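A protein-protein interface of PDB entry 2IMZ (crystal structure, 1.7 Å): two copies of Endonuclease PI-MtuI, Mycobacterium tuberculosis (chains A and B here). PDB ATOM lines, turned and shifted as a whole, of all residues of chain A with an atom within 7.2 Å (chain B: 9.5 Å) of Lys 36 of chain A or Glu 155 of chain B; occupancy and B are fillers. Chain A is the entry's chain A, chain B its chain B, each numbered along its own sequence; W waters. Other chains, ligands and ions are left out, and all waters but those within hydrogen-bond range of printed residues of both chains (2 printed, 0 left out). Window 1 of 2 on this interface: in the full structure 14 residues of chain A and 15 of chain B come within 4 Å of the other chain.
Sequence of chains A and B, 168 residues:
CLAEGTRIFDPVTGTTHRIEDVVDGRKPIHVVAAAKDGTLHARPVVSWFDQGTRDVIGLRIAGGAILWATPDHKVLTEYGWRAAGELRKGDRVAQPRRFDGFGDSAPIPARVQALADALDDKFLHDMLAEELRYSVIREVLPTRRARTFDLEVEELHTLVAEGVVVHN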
ATOM      1  N   ALA A  34       4.116  17.521 -16.646  1.00  0.00           N
ATOM      2  CA  ALA A  34       4.805  16.375 -17.223  1.00  0.00           C
ATOM      3  C   ALA A  34       5.930  15.898 -16.316  1.00  0.00           C
ATOM      4  O   ALA A  34       6.715  16.702 -15.814  1.00  0.00           O
ATOM      5  CB  ALA A  34       5.370  16.742 -18.594  1.00  0.00           C
ATOM      6  N   ALA A  35       6.003  14.584 -16.116  1.00  0.00           N
ATOM      7  CA  ALA A  35       7.040  13.977 -15.290  1.00  0.00           C
ATOM      8  C   ALA A  35       8.232  13.633 -16.181  1.00  0.00           C
ATOM      9  O   ALA A  35       8.154  13.751 -17.404  1.00  0.00           O
ATOM     10  CB  ALA A  35       6.501  12.719 -14.612  1.00  0.00           C
ATOM     11  N   LYS A  36       9.332  13.200 -15.571  1.00  0.00           N
ATOM     12  CA  LYS A  36      10.538  12.869 -16.324  1.00  0.00           C
ATOM     13  C   LYS A  36      10.324  11.876 -17.464  1.00  0.00           C
ATOM     14  O   LYS A  36      10.931  12.009 -18.532  1.00  0.00           O
ATOM     15  CB  LYS A  36      11.612  12.321 -15.383  1.00  0.00           C
ATOM     16  CG  LYS A  36      12.874  11.866 -16.103  1.00  0.00           C
ATOM     17  CD  LYS A  36      13.895  11.277 -15.145  1.00  0.00           C
ATOM     18  CE  LYS A  36      13.346  10.061 -14.419  1.00  0.00           C
ATOM     19  NZ  LYS A  36      14.381   9.422 -13.558  1.00  0.00           N
ATOM     20  N   ASP A  37       9.469  10.883 -17.238  1.00  0.00           N
ATOM     21  CA  ASP A  37       9.207   9.865 -18.254  1.00  0.00           C
ATOM     22  C   ASP A  37       8.156  10.263 -19.287  1.00  0.00           C
ATOM     23  O   ASP A  37       7.801   9.464 -20.154  1.00  0.00           O
ATOM     24  CB  ASP A  37       8.801   8.542 -17.591  1.00  0.00           C
ATOM     25  CG  ASP A  37       7.591   8.681 -16.683  1.00  0.00           C
ATOM     26  OD1 ASP A  37       6.914   9.731 -16.733  1.00  0.00           O
ATOM     27  OD2 ASP A  37       7.312   7.732 -15.920  1.00  0.00           O
ATOM     28  N   GLY A  38       7.659  11.491 -19.201  1.00  0.00           N
ATOM     29  CA  GLY A  38       6.665  11.937 -20.162  1.00  0.00           C
ATOM     30  C   GLY A  38       5.225  11.719 -19.736  1.00  0.00           C
ATOM     31  O   GLY A  38       4.302  12.128 -20.444  1.00  0.00           O
ATOM     32  N   THR A  39       5.014  11.070 -18.595  1.00  0.00           N
ATOM     33  CA  THR A  39       3.653  10.852 -18.123  1.00  0.00           C
ATOM     34  C   THR A  39       3.129  12.170 -17.563  1.00  0.00           C
ATOM     35  O   THR A  39       3.908  13.015 -17.118  1.00  0.00           O
ATOM     36  CB  THR A  39       3.584   9.753 -17.034  1.00  0.00           C
ATOM     37  OG1 THR A  39       4.495  10.056 -15.973  1.00  0.00           O
ATOM     38  CG2 THR A  39       3.941   8.395 -17.630  1.00  0.00           C
ATOM     39  N   HIS A  41       0.550  14.414 -14.943  1.00  0.00           N
ATOM     40  CA  HIS A  41      -0.083  14.374 -13.629  1.00  0.00           C
ATOM     41  C   HIS A  41      -0.656  15.719 -13.226  1.00  0.00           C
ATOM     42  O   HIS A  41      -0.174  16.765 -13.654  1.00  0.00           O
ATOM     43  CB  HIS A  41       0.937  13.963 -12.565  1.00  0.00           C
ATOM     44  CG  HIS A  41       1.683  12.709 -12.890  1.00  0.00           C
ATOM     45  ND1 HIS A  41       2.650  12.649 -13.870  1.00  0.00           N
ATOM     46  CD2 HIS A  41       1.593  11.461 -12.373  1.00  0.00           C
ATOM     47  CE1 HIS A  41       3.124  11.419 -13.941  1.00  0.00           C
ATOM     48  NE2 HIS A  41       2.499  10.678 -13.044  1.00  0.00           N
ATOM     49  N   TRP A  81      14.405  20.430 -23.531  1.00  0.00           N
ATOM     50  CA  TRP A  81      14.032  21.832 -23.388  1.00  0.00           C
ATOM     51  C   TRP A  81      14.711  22.734 -24.409  1.00  0.00           C
ATOM     52  O   TRP A  81      15.912  22.622 -24.663  1.00  0.00           O
ATOM     53  CB  TRP A  81      14.358  22.319 -21.972  1.00  0.00           C
ATOM     54  CG  TRP A  81      13.615  21.565 -20.923  1.00  0.00           C
ATOM     55  CD1 TRP A  81      14.098  20.565 -20.132  1.00  0.00           C
ATOM     56  CD2 TRP A  81      12.229  21.702 -20.597  1.00  0.00           C
ATOM     57  NE1 TRP A  81      13.096  20.066 -19.333  1.00  0.00           N
ATOM     58  CE2 TRP A  81      11.938  20.748 -19.599  1.00  0.00           C
ATOM     59  CE3 TRP A  81      11.203  22.540 -21.056  1.00  0.00           C
ATOM     60  CZ2 TRP A  81      10.658  20.604 -19.048  1.00  0.00           C
ATOM     61  CZ3 TRP A  81       9.930  22.397 -20.510  1.00  0.00           C
ATOM     62  CH2 TRP A  81       9.671  21.435 -19.514  1.00  0.00           C
ATOM     63  N   GLU A 155       6.526  19.819  -7.177  1.00  0.00           N
ATOM     64  CA  GLU A 155       7.273  18.637  -7.603  1.00  0.00           C
ATOM     65  C   GLU A 155       7.807  18.521  -9.033  1.00  0.00           C
ATOM     66  O   GLU A 155       9.015  18.376  -9.236  1.00  0.00           O
ATOM     67  CB  GLU A 155       6.457  17.372  -7.276  1.00  0.00           C
ATOM     68  CG  GLU A 155       7.161  16.063  -7.656  1.00  0.00           C
ATOM     69  CD  GLU A 155       6.316  14.822  -7.397  1.00  0.00           C
ATOM     70  OE1 GLU A 155       5.105  14.840  -7.696  1.00  0.00           O
ATOM     71  OE2 GLU A 155       6.872  13.814  -6.909  1.00  0.00           O
ATOM     72  N   LEU A 156       6.921  18.585 -10.022  1.00  0.00           N
ATOM     73  CA  LEU A 156       7.333  18.396 -11.408  1.00  0.00           C
ATOM     74  C   LEU A 156       7.913  19.586 -12.165  1.00  0.00           C
ATOM     75  O   LEU A 156       8.580  19.399 -13.179  1.00  0.00           O
ATOM     76  CB  LEU A 156       6.177  17.774 -12.191  1.00  0.00           C
ATOM     77  CG  LEU A 156       5.722  16.448 -11.562  1.00  0.00           C
ATOM     78  CD1 LEU A 156       4.565  15.853 -12.355  1.00  0.00           C
ATOM     79  CD2 LEU A 156       6.896  15.476 -11.530  1.00  0.00           C
ATOM     80  N   HIS A 157       7.659  20.797 -11.686  1.00  0.00           N
ATOM     81  CA  HIS A 157       8.220  21.988 -12.313  1.00  0.00           C
ATOM     82  C   HIS A 157       7.892  22.214 -13.782  1.00  0.00           C
ATOM     83  O   HIS A 157       8.682  22.812 -14.514  1.00  0.00           O
ATOM     84  CB  HIS A 157       9.742  21.985 -12.130  1.00  0.00           C
ATOM     85  CG  HIS A 157      10.172  22.209 -10.716  1.00  0.00           C
ATOM     86  ND1 HIS A 157      10.213  23.462 -10.144  1.00  0.00           N
ATOM     87  CD2 HIS A 157      10.525  21.337  -9.739  1.00  0.00           C
ATOM     88  CE1 HIS A 157      10.570  23.352  -8.875  1.00  0.00           C
ATOM     89  NE2 HIS A 157      10.763  22.073  -8.605  1.00  0.00           N
ATOM     90  N   VAL B  31      24.984  17.102 -10.377  1.00  0.00           N
ATOM     91  CA  VAL B  31      24.885  18.138  -9.356  1.00  0.00           C
ATOM     92  C   VAL B  31      24.120  17.606  -8.154  1.00  0.00           C
ATOM     93  O   VAL B  31      23.518  16.533  -8.208  1.00  0.00           O
ATOM     94  CB  VAL B  31      24.134  19.394  -9.891  1.00  0.00           C
ATOM     95  CG1 VAL B  31      24.818  19.919 -11.152  1.00  0.00           C
ATOM     96  CG2 VAL B  31      22.666  19.059 -10.164  1.00  0.00           C
ATOM     97  N   ALA B  33      21.023  17.793  -6.291  1.00  0.00           N
ATOM     98  CA  ALA B  33      19.677  18.306  -6.523  1.00  0.00           C
ATOM     99  C   ALA B  33      18.782  18.018  -5.332  1.00  0.00           C
ATOM    100  O   ALA B  33      18.968  17.030  -4.629  1.00  0.00           O
ATOM    101  CB  ALA B  33      19.083  17.680  -7.783  1.00  0.00           C
ATOM    102  N   ALA B  34      17.805  18.889  -5.107  1.00  0.00           N
ATOM    103  CA  ALA B  34      16.894  18.714  -3.987  1.00  0.00           C
ATOM    104  C   ALA B  34      15.541  18.225  -4.475  1.00  0.00           C
ATOM    105  O   ALA B  34      14.983  18.772  -5.425  1.00  0.00           O
ATOM    106  CB  ALA B  34      16.730  20.030  -3.236  1.00  0.00           C
ATOM    107  N   ALA B  35      15.030  17.186  -3.824  1.00  0.00           N
ATOM    108  CA  ALA B  35      13.732  16.624  -4.169  1.00  0.00           C
ATOM    109  C   ALA B  35      12.673  17.391  -3.388  1.00  0.00           C
ATOM    110  O   ALA B  35      12.999  18.169  -2.490  1.00  0.00           O
ATOM    111  CB  ALA B  35      13.686  15.147  -3.809  1.00  0.00           C
ATOM    112  N   LYS B  36      11.410  17.163  -3.732  1.00  0.00           N
ATOM    113  CA  LYS B  36      10.288  17.831  -3.083  1.00  0.00           C
ATOM    114  C   LYS B  36      10.309  17.736  -1.559  1.00  0.00           C
ATOM    115  O   LYS B  36       9.917  18.679  -0.872  1.00  0.00           O
ATOM    116  CB  LYS B  36       8.973  17.242  -3.595  1.00  0.00           C
ATOM    117  CG  LYS B  36       7.734  17.895  -3.006  1.00  0.00           C
ATOM    118  CD  LYS B  36       6.656  16.868  -2.697  1.00  0.00           C
ATOM    119  CE  LYS B  36       6.299  16.033  -3.913  1.00  0.00           C
ATOM    120  NZ  LYS B  36       5.277  15.001  -3.579  1.00  0.00           N
ATOM    121  N   HIS B  41      19.748  14.397  -4.061  1.00  0.00           N
ATOM    122  CA  HIS B  41      20.032  13.343  -5.031  1.00  0.00           C
ATOM    123  C   HIS B  41      20.913  13.835  -6.168  1.00  0.00           C
ATOM    124  O   HIS B  41      20.759  14.961  -6.636  1.00  0.00           O
ATOM    125  CB  HIS B  41      18.714  12.834  -5.609  1.00  0.00           C
ATOM    126  CG  HIS B  41      17.750  12.373  -4.567  1.00  0.00           C
ATOM    127  ND1 HIS B  41      17.730  11.079  -4.094  1.00  0.00           N
ATOM    128  CD2 HIS B  41      16.833  13.054  -3.839  1.00  0.00           C
ATOM    129  CE1 HIS B  41      16.843  10.984  -3.118  1.00  0.00           C
ATOM    130  NE2 HIS B  41      16.287  12.169  -2.943  1.00  0.00           N
ATOM    131  N   ALA B  42      21.820  12.977  -6.627  1.00  0.00           N
ATOM    132  CA  ALA B  42      22.711  13.336  -7.721  1.00  0.00           C
ATOM    133  C   ALA B  42      21.943  13.225  -9.029  1.00  0.00           C
ATOM    134  O   ALA B  42      21.378  12.175  -9.345  1.00  0.00           O
ATOM    135  CB  ALA B  42      23.926  12.405  -7.742  1.00  0.00           C
ATOM    136  N   ARG B  43      21.909  14.318  -9.780  1.00  0.00           N
ATOM    137  CA  ARG B  43      21.212  14.333 -11.061  1.00  0.00           C
ATOM    138  C   ARG B  43      22.097  14.971 -12.117  1.00  0.00           C
ATOM    139  O   ARG B  43      22.826  15.929 -11.847  1.00  0.00           O
ATOM    140  CB  ARG B  43      19.885  15.087 -10.935  1.00  0.00           C
ATOM    141  CG  ARG B  43      18.830  14.334 -10.128  1.00  0.00           C
ATOM    142  CD  ARG B  43      18.376  13.078 -10.874  1.00  0.00           C
ATOM    143  NE  ARG B  43      17.307  12.356 -10.185  1.00  0.00           N
ATOM    144  CZ  ARG B  43      17.491  11.438  -9.236  1.00  0.00           C
ATOM    145  NH1 ARG B  43      18.714  11.107  -8.836  1.00  0.00           N
ATOM    146  NH2 ARG B  43      16.441  10.834  -8.698  1.00  0.00           N
ATOM    147  N   PRO B  44      22.047  14.444 -13.345  1.00  0.00           N
ATOM    148  CA  PRO B  44      22.857  14.968 -14.440  1.00  0.00           C
ATOM    149  C   PRO B  44      22.330  16.233 -15.107  1.00  0.00           C
ATOM    150  O   PRO B  44      21.124  16.459 -15.173  1.00  0.00           O
ATOM    151  CB  PRO B  44      22.891  13.798 -15.413  1.00  0.00           C
ATOM    152  CG  PRO B  44      21.513  13.244 -15.273  1.00  0.00           C
ATOM    153  CD  PRO B  44      21.313  13.236 -13.768  1.00  0.00           C
ATOM    154  N   VAL B  45      23.255  17.054 -15.593  1.00  0.00           N
ATOM    155  CA  VAL B  45      22.908  18.266 -16.320  1.00  0.00           C
ATOM    156  C   VAL B  45      22.599  17.768 -17.733  1.00  0.00           C
ATOM    157  O   VAL B  45      23.383  17.011 -18.310  1.00  0.00           O
ATOM    158  CB  VAL B  45      24.099  19.249 -16.366  1.00  0.00           C
ATOM    159  CG1 VAL B  45      23.812  20.377 -17.342  1.00  0.00           C
ATOM    160  CG2 VAL B  45      24.357  19.814 -14.971  1.00  0.00           C
ATOM    161  N   VAL B  46      21.454  18.175 -18.275  1.00  0.00           N
ATOM    162  CA  VAL B  46      21.036  17.743 -19.608  1.00  0.00           C
ATOM    163  C   VAL B  46      20.922  18.878 -20.628  1.00  0.00           C
ATOM    164  O   VAL B  46      20.783  18.630 -21.829  1.00  0.00           O
ATOM    165  CB  VAL B  46      19.686  16.993 -19.541  1.00  0.00           C
ATOM    166  CG1 VAL B  46      19.858  15.685 -18.783  1.00  0.00           C
ATOM    167  CG2 VAL B  46      18.640  17.859 -18.860  1.00  0.00           C
ATOM    168  N   GLU B 152      19.959  22.808 -17.039  1.00  0.00           N
ATOM    169  CA  GLU B 152      18.775  22.003 -16.791  1.00  0.00           C
ATOM    170  C   GLU B 152      19.288  20.741 -16.113  1.00  0.00           C
ATOM    171  O   GLU B 152      20.200  20.078 -16.614  1.00  0.00           O
ATOM    172  CB  GLU B 152      18.037  21.650 -18.084  1.00  0.00           C
ATOM    173  CG  GLU B 152      17.048  22.712 -18.527  1.00  0.00           C
ATOM    174  CD  GLU B 152      16.124  23.165 -17.403  1.00  0.00           C
ATOM    175  OE1 GLU B 152      15.417  22.319 -16.804  1.00  0.00           O
ATOM    176  OE2 GLU B 152      16.102  24.381 -17.119  1.00  0.00           O
ATOM    177  N   VAL B 153      18.706  20.441 -14.957  1.00  0.00           N
ATOM    178  CA  VAL B 153      19.071  19.285 -14.148  1.00  0.00           C
ATOM    179  C   VAL B 153      17.943  18.281 -14.283  1.00  0.00           C
ATOM    180  O   VAL B 153      16.801  18.568 -13.931  1.00  0.00           O
ATOM    181  CB  VAL B 153      19.236  19.707 -12.668  1.00  0.00           C
ATOM    182  CG1 VAL B 153      19.510  18.490 -11.783  1.00  0.00           C
ATOM    183  CG2 VAL B 153      20.374  20.717 -12.558  1.00  0.00           C
ATOM    184  N   GLU B 154      18.268  17.101 -14.796  1.00  0.00           N
ATOM    185  CA  GLU B 154      17.260  16.081 -15.018  1.00  0.00           C
ATOM    186  C   GLU B 154      16.360  15.760 -13.832  1.00  0.00           C
ATOM    187  O   GLU B 154      16.822  15.626 -12.690  1.00  0.00           O
ATOM    188  CB  GLU B 154      17.928  14.799 -15.527  1.00  0.00           C
ATOM    189  CG  GLU B 154      16.954  13.684 -15.862  1.00  0.00           C
ATOM    190  CD  GLU B 154      17.604  12.579 -16.667  1.00  0.00           C
ATOM    191  OE1 GLU B 154      17.701  12.722 -17.904  1.00  0.00           O
ATOM    192  OE2 GLU B 154      18.029  11.576 -16.063  1.00  0.00           O
ATOM    193  N   GLU B 155      15.065  15.661 -14.135  1.00  0.00           N
ATOM    194  CA  GLU B 155      14.006  15.319 -13.191  1.00  0.00           C
ATOM    195  C   GLU B 155      13.643  16.285 -12.063  1.00  0.00           C
ATOM    196  O   GLU B 155      12.485  16.688 -11.942  1.00  0.00           O
ATOM    197  CB  GLU B 155      14.279  13.935 -12.584  1.00  0.00           C
ATOM    198  CG  GLU B 155      13.257  13.511 -11.527  1.00  0.00           C
ATOM    199  CD  GLU B 155      13.550  12.146 -10.926  1.00  0.00           C
ATOM    200  OE1 GLU B 155      14.727  11.869 -10.621  1.00  0.00           O
ATOM    201  OE2 GLU B 155      12.601  11.353 -10.743  1.00  0.00           O
ATOM    202  N   LEU B 156      14.620  16.660 -11.244  1.00  0.00           N
ATOM    203  CA  LEU B 156      14.347  17.520 -10.098  1.00  0.00           C
ATOM    204  C   LEU B 156      14.348  19.028 -10.317  1.00  0.00           C
ATOM    205  O   LEU B 156      13.776  19.766  -9.517  1.00  0.00           O
ATOM    206  CB  LEU B 156      15.290  17.150  -8.950  1.00  0.00           C
ATOM    207  CG  LEU B 156      15.190  15.676  -8.543  1.00  0.00           C
ATOM    208  CD1 LEU B 156      16.129  15.413  -7.376  1.00  0.00           C
ATOM    209  CD2 LEU B 156      13.753  15.328  -8.160  1.00  0.00           C
ATOM    210  N   HIS B 157      14.981  19.484 -11.390  1.00  0.00           N
ATOM    211  CA  HIS B 157      15.013  20.908 -11.720  1.00  0.00           C
ATOM    212  C   HIS B 157      15.556  21.837 -10.637  1.00  0.00           C
ATOM    213  O   HIS B 157      15.162  22.996 -10.563  1.00  0.00           O
ATOM    214  CB  HIS B 157      13.606  21.367 -12.124  1.00  0.00           C
ATOM    215  CG  HIS B 157      13.141  20.796 -13.429  1.00  0.00           C
ATOM    216  ND1 HIS B 157      13.440  21.376 -14.643  1.00  0.00           N
ATOM    217  CD2 HIS B 157      12.434  19.675 -13.709  1.00  0.00           C
ATOM    218  CE1 HIS B 157      12.936  20.638 -15.616  1.00  0.00           C
ATOM    219  NE2 HIS B 157      12.321  19.600 -15.077  1.00  0.00           N
ATOM    220  N   THR B 158      16.456  21.330  -9.801  1.00  0.00           N
ATOM    221  CA  THR B 158      17.058  22.138  -8.743  1.00  0.00           C
ATOM    222  C   THR B 158      18.526  21.760  -8.616  1.00  0.00           C
ATOM    223  O   THR B 158      18.962  20.743  -9.150  1.00  0.00           O
ATOM    224  CB  THR B 158      16.386  21.901  -7.375  1.00  0.00           C
ATOM    225  OG1 THR B 158      16.578  20.537  -6.984  1.00  0.00           O
ATOM    226  CG2 THR B 158      14.897  22.203  -7.444  1.00  0.00           C
ATOM    227  N   LEU B 159      19.292  22.584  -7.914  1.00  0.00           N
ATOM    228  CA  LEU B 159      20.708  22.304  -7.725  1.00  0.00           C
ATOM    229  C   LEU B 159      21.270  23.198  -6.636  1.00  0.00           C
ATOM    230  O   LEU B 159      20.724  24.264  -6.349  1.00  0.00           O
ATOM    231  CB  LEU B 159      21.498  22.554  -9.019  1.00  0.00           C
ATOM    232  CG  LEU B 159      21.714  24.019  -9.419  1.00  0.00           C
ATOM    233  CD1 LEU B 159      22.901  24.133 -10.363  1.00  0.00           C
ATOM    234  CD2 LEU B 159      20.447  24.569 -10.066  1.00  0.00           C
ATOM    235  N1  SNN B 168      15.693  24.088 -13.960  1.00  0.00           N
ATOM    236  C   SNN B 168      15.698  25.276 -13.356  1.00  0.00           C
ATOM    237  CA  SNN B 168      16.857  25.317 -12.373  1.00  0.00           C
ATOM    238  N   SNN B 168      16.336  25.490 -11.005  1.00  0.00           N
ATOM    239  C4  SNN B 168      17.529  23.952 -12.525  1.00  0.00           C
ATOM    240  C5  SNN B 168      16.679  23.263 -13.569  1.00  0.00           C
ATOM    241  O   SNN B 168      14.909  26.167 -13.559  1.00  0.00           O
ATOM    242  O5  SNN B 168      16.861  22.146 -13.983  1.00  0.00           O
HETATM  243  O   HOH W   1       3.596  15.879  -5.380  1.00  0.00           O
HETATM  244  O   HOH W   2      10.341  15.255  -9.729  1.00  0.00           O
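Lys 36 of chain A touches Glu 154 of chain B (CD to CG, 3.96 Å). Trp 81 of chain A touches Glu 152 of chain B (CD1 to CG, 3.99 Å). NE1 of Trp 81 of chain A touches CE1 of His 157 of chain B, at 3.8 Å. O of Leu 156 of chain A touches CD2 of His 157 of chain B, at 3.9 Å. CD2 of His 157 of chain A touches O of Leu 156 of chain B (3.6 Å). His 157 of chain A touches His 157 of chain B (CG to CB, 3.8 Å).
Lys 36 of chain A touches Glu 155 of chain B, and with the chains exchanged Glu 155 of chain A touches Lys 36 of chain B. Leu 156 of chain A touches His 157 of chain B, and with the chains exchanged His 157 of chain A touches Leu 156 of chain B. His 157 of chain A touches its own counterpart, His 157 of chain B. Of the 8 pairs that touch across the chains among the printed residues, 5 have their exchanged pair printed and touching as well.
Water W1 bridges the side-chain amino group (NZ) of Lys 36 of chain B (2.6 Å) and the side-chain carboxylate (OE1) of Glu 155 of chain A (3.0 Å). Water W2 lies within hydrogen-bond range of the backbone carbonyl oxygen (O) of Glu 155 of chain B (3.4 Å) and the backbone carbonyl oxygen (O) of Glu 155 of chain A (3.4 Å).
The backbone carbonyl oxygen of Glu 152 of chain B is in hydrogen-bond range of the backbone NH of Val 46 of chain B (2.8 Å). The side-chain carboxylate (OE1) of Glu 155 of chain B is in salt-bridge range of the guanidinium group (NE) of Arg 43 of chain B (2.7 Å). The backbone NH (N) of Glu 154 of chain B lies within hydrogen-bond range of the backbone carbonyl oxygen (O) of Pro 44 of chain B (3.0 Å).
The side-chain carboxylate of Glu 155 of chain B lies within salt-bridge range of the side-chain amino group of Lys 36 of chain A, 3.8 Å away. The side-chain carboxylate (OE2) of Glu 155 of chain A is in salt-bridge range of the side-chain amino group (NZ) of Lys 36 of chain B (3.9 Å).
Lys 36 of chain A touches just these residues of chain B: Glu 154 (3.96 Å) and Glu 155 (3.7 Å). Of the printed residues of chain A, Glu 155 of chain B touches Lys 36 (3.7 Å). No residue of chain B comes within 4 Å of Ala 35 of chain A. Of the printed residues of chain A, Leu 156 of chain B touches His 157. Of the printed residues of chain A, Glu 152 of chain B touches Trp 81 (3.99 Å). Of the printed residues of chain B, Trp 81 of chain A touches Glu 152 (3.99 Å) and His 157 (3.8 Å). Of the printed residues of chain A, His 157 of chain B touches Trp 81, Leu 156 and His 157. The nearest printed residue of chain B that does not touch Trp 81 of chain A is Val 46 of chain B (5.4 Å).
Printed residues of chain B that touch a printed residue of chain A: Lys 36, Glu 152, Glu 154, Glu 155, Leu 156 and His 157. Hydrophobic or aromatic side chains of chain B within 4 Å of the printed part of chain A: His 157. Of the 11 printed residues of chain A, 5 touch a printed residue of chain B. Hydrophobic or aromatic side chains of chain A within 4 Å of the printed part of chain B: Trp 81 and His 157. Along chain A the printed residues that touch a printed residue of chain B span positions 36 to 157. Among the printed residues, 8 pairs touch across the chains. Among the printed residues, Asp or Glu carboxylates within 4 Å of a Lys or Arg side-chain nitrogen of the other chain: Lys 36 of chain A with Glu 155 of chain B (3.8 Å) and Glu 155 of chain A with Lys 36 of chain B (3.9 Å).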
